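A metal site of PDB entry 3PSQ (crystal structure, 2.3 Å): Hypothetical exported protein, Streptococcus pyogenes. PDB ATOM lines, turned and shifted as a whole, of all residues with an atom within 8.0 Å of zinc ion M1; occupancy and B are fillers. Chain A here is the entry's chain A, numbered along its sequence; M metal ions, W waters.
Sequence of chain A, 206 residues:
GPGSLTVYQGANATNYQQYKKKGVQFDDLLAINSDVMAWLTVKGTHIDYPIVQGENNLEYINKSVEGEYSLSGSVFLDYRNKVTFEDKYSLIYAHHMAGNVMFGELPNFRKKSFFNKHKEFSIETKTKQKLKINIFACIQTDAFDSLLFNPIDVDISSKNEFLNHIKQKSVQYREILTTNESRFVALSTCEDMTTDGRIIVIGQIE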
ATOM      1  N   ASN A  33      -1.332   4.112  14.360  1.00  0.00           N
ATOM      2  CA  ASN A  33      -0.375   4.935  15.044  1.00  0.00           C
ATOM      3  C   ASN A  33      -0.447   4.599  16.524  1.00  0.00           C
ATOM      4  O   ASN A  33      -1.396   4.982  17.227  1.00  0.00           O
ATOM      5  CB  ASN A  33      -0.702   6.417  14.762  1.00  0.00           C
ATOM      6  CG  ASN A  33       0.222   7.421  15.491  1.00  0.00           C
ATOM      7  OD1 ASN A  33       1.246   7.044  16.062  1.00  0.00           O
ATOM      8  ND2 ASN A  33      -0.163   8.672  15.487  1.00  0.00           N
ATOM      9  N   SER A  34       0.566   3.905  17.011  1.00  0.00           N
ATOM     10  CA  SER A  34       0.630   3.541  18.431  1.00  0.00           C
ATOM     11  C   SER A  34       0.642   4.743  19.388  1.00  0.00           C
ATOM     12  O   SER A  34       0.408   4.560  20.605  1.00  0.00           O
ATOM     13  CB  SER A  34       1.823   2.627  18.685  1.00  0.00           C
ATOM     14  OG  SER A  34       3.041   3.332  18.457  1.00  0.00           O
ATOM     15  N   ASP A  35       0.893   5.954  18.877  1.00  0.00           N
ATOM     16  CA  ASP A  35       0.693   7.179  19.691  1.00  0.00           C
ATOM     17  C   ASP A  35      -0.786   7.457  20.051  1.00  0.00           C
ATOM     18  O   ASP A  35      -1.066   8.146  21.032  1.00  0.00           O
ATOM     19  CB  ASP A  35       1.231   8.419  18.967  1.00  0.00           C
ATOM     20  CG  ASP A  35       2.749   8.513  18.973  1.00  0.00           C
ATOM     21  OD1 ASP A  35       3.429   7.594  19.446  1.00  0.00           O
ATOM     22  OD2 ASP A  35       3.263   9.550  18.487  1.00  0.00           O
ATOM     23  N   VAL A  36      -1.716   6.979  19.223  1.00  0.00           N
ATOM     24  CA  VAL A  36      -3.152   7.132  19.499  1.00  0.00           C
ATOM     25  C   VAL A  36      -3.511   6.389  20.812  1.00  0.00           C
ATOM     26  O   VAL A  36      -3.162   5.225  20.958  1.00  0.00           O
ATOM     27  CB  VAL A  36      -4.030   6.662  18.302  1.00  0.00           C
ATOM     28  CG1 VAL A  36      -5.535   6.737  18.653  1.00  0.00           C
ATOM     29  CG2 VAL A  36      -3.732   7.518  17.001  1.00  0.00           C
ATOM     30  N   VAL A  52      -3.803  11.738  20.787  1.00  0.00           N
ATOM     31  CA  VAL A  52      -2.507  11.096  20.755  1.00  0.00           C
ATOM     32  C   VAL A  52      -1.687  11.515  21.944  1.00  0.00           C
ATOM     33  O   VAL A  52      -1.956  12.546  22.577  1.00  0.00           O
ATOM     34  CB  VAL A  52      -1.707  11.438  19.476  1.00  0.00           C
ATOM     35  CG1 VAL A  52      -2.340  10.780  18.258  1.00  0.00           C
ATOM     36  CG2 VAL A  52      -1.567  12.958  19.311  1.00  0.00           C
ATOM     37  N   GLN A  53      -0.642  10.726  22.219  1.00  0.00           N
ATOM     38  CA  GLN A  53       0.417  11.198  23.071  1.00  0.00           C
ATOM     39  C   GLN A  53       1.728  11.086  22.318  1.00  0.00           C
ATOM     40  O   GLN A  53       2.077  10.006  21.818  1.00  0.00           O
ATOM     41  CB  GLN A  53       0.522  10.392  24.360  1.00  0.00           C
ATOM     42  CG  GLN A  53       1.708  10.846  25.239  1.00  0.00           C
ATOM     43  CD  GLN A  53       1.827   9.998  26.492  1.00  0.00           C
ATOM     44  OE1 GLN A  53       2.158   8.813  26.420  1.00  0.00           O
ATOM     45  NE2 GLN A  53       1.564  10.600  27.647  1.00  0.00           N
ATOM     46  N   GLY A  54       2.475  12.203  22.254  1.00  0.00           N
ATOM     47  CA  GLY A  54       3.779  12.155  21.604  1.00  0.00           C
ATOM     48  C   GLY A  54       4.906  11.839  22.569  1.00  0.00           C
ATOM     49  O   GLY A  54       4.679  11.744  23.787  1.00  0.00           O
ATOM     50  N   GLU A  55       6.131  11.724  22.032  1.00  0.00           N
ATOM     51  CA  GLU A  55       7.341  11.467  22.850  1.00  0.00           C
ATOM     52  C   GLU A  55       7.808  12.746  23.506  1.00  0.00           C
ATOM     53  O   GLU A  55       8.628  12.707  24.433  1.00  0.00           O
ATOM     54  CB  GLU A  55       8.452  10.830  22.036  1.00  0.00           C
ATOM     55  CG  GLU A  55       8.086   9.434  21.443  1.00  0.00           C
ATOM     56  CD  GLU A  55       7.218   9.531  20.174  1.00  0.00           C
ATOM     57  OE1 GLU A  55       7.788   9.832  19.108  1.00  0.00           O
ATOM     58  OE2 GLU A  55       5.985   9.268  20.229  1.00  0.00           O
ATOM     59  N   ASN A  56       7.262  13.860  23.028  1.00  0.00           N
ATOM     60  CA  ASN A  56       7.479  15.188  23.585  1.00  0.00           C
ATOM     61  C   ASN A  56       6.254  16.023  23.254  1.00  0.00           C
ATOM     62  O   ASN A  56       5.359  15.535  22.563  1.00  0.00           O
ATOM     63  CB  ASN A  56       8.751  15.835  22.987  1.00  0.00           C
ATOM     64  CG  ASN A  56       8.691  15.970  21.455  1.00  0.00           C
ATOM     65  OD1 ASN A  56       7.882  16.719  20.940  1.00  0.00           O
ATOM     66  ND2 ASN A  56       9.528  15.218  20.733  1.00  0.00           N
ATOM     67  N   GLU A  59       5.935  17.416  19.053  1.00  0.00           N
ATOM     68  CA  GLU A  59       5.735  16.449  17.994  1.00  0.00           C
ATOM     69  C   GLU A  59       4.467  16.612  17.107  1.00  0.00           C
ATOM     70  O   GLU A  59       4.505  16.372  15.879  1.00  0.00           O
ATOM     71  CB  GLU A  59       5.824  15.017  18.549  1.00  0.00           C
ATOM     72  CG  GLU A  59       5.430  13.876  17.527  1.00  0.00           C
ATOM     73  CD  GLU A  59       5.490  12.508  18.166  1.00  0.00           C
ATOM     74  OE1 GLU A  59       5.639  12.451  19.397  1.00  0.00           O
ATOM     75  OE2 GLU A  59       5.366  11.487  17.456  1.00  0.00           O
ATOM     76  N   TYR A  60       3.369  16.991  17.733  1.00  0.00           N
ATOM     77  CA  TYR A  60       2.087  17.097  17.051  1.00  0.00           C
ATOM     78  C   TYR A  60       1.687  18.521  16.629  1.00  0.00           C
ATOM     79  O   TYR A  60       0.547  18.749  16.286  1.00  0.00           O
ATOM     80  CB  TYR A  60       0.945  16.365  17.832  1.00  0.00           C
ATOM     81  CG  TYR A  60       1.069  14.867  17.617  1.00  0.00           C
ATOM     82  CD1 TYR A  60       0.540  14.280  16.503  1.00  0.00           C
ATOM     83  CD2 TYR A  60       1.836  14.079  18.475  1.00  0.00           C
ATOM     84  CE1 TYR A  60       0.729  12.937  16.246  1.00  0.00           C
ATOM     85  CE2 TYR A  60       2.016  12.719  18.234  1.00  0.00           C
ATOM     86  CZ  TYR A  60       1.463  12.160  17.122  1.00  0.00           C
ATOM     87  OH  TYR A  60       1.622  10.815  16.833  1.00  0.00           O
ATOM     88  N   LYS A  63       1.710  17.389  12.797  1.00  0.00           N
ATOM     89  CA  LYS A  63       1.497  15.977  12.563  1.00  0.00           C
ATOM     90  C   LYS A  63       0.048  15.590  12.868  1.00  0.00           C
ATOM     91  O   LYS A  63      -0.522  16.016  13.871  1.00  0.00           O
ATOM     92  CB  LYS A  63       2.460  15.187  13.455  1.00  0.00           C
ATOM     93  CG  LYS A  63       2.534  13.702  13.160  1.00  0.00           C
ATOM     94  CD  LYS A  63       3.704  13.238  14.012  1.00  0.00           C
ATOM     95  CE  LYS A  63       3.984  11.789  13.881  1.00  0.00           C
ATOM     96  NZ  LYS A  63       5.043  11.458  14.904  1.00  0.00           N
ATOM     97  N   GLY A  67      -0.363  10.132  11.859  1.00  0.00           N
ATOM     98  CA  GLY A  67       1.085  10.108  11.897  1.00  0.00           C
ATOM     99  C   GLY A  67       1.780  10.732  10.708  1.00  0.00           C
ATOM    100  O   GLY A  67       2.975  10.498  10.476  1.00  0.00           O
HETATM  101 ZN    ZN M   1       5.270   9.741  18.327  1.00  0.00          ZN
HETATM  102 ZN    ZN M   2       4.400   6.899  23.495  1.00  0.00          ZN
HETATM  103  O   HOH W   1       5.579   8.351  16.851  1.00  0.00           O
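The side-chain amino group (NZ) of Lys 63 lies close to the side-chain carboxylate (OE2) of Glu 59 (2.6 Å).
The backbone NH of Glu 59 is in hydrogen-bond range of the side-chain amide oxygen of Asn 56, 2.8 Å away.
The side-chain hydroxyl (OH) of Tyr 60 sits close to the side-chain carboxylate (OD2) of Asp 35, at 2.7 Å.
The backbone NH (N) of Gln 53 lies within hydrogen-bond range of the backbone carbonyl oxygen (O) of Asp 35 (2.9 Å).
The side-chain amide oxygen of Asn 33 sits close to the backbone NH of Asp 35 (3.0 Å).
Lys 63 touches zinc ion M1 (NZ to ZN, 3.8 Å).
Within 4 Å of zinc ion M1: Asp 35, Glu 55, Glu 59 and Lys 63.
The nearest printed residue that does not touch zinc ion M1 is Tyr 60 (4.1 Å).
Zinc ion M1 is bound by the side-chain carboxylate (OE2) of Glu 59, the side-chain carboxylate (OD2) of Asp 35, water W1 and the side-chain carboxylate (OE2) of Glu 55.
Zinc ion M1 has four donor atoms within binding distance.
Slightly farther from zinc ion M1 lies the side-chain carboxylate (OE1) of Glu 55 (2.6 Å).
Water W1 lies within hydrogen-bond range of OD1 of Asp 35 (3.5 Å) and OE1 of Glu 55 (3.5 Å).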
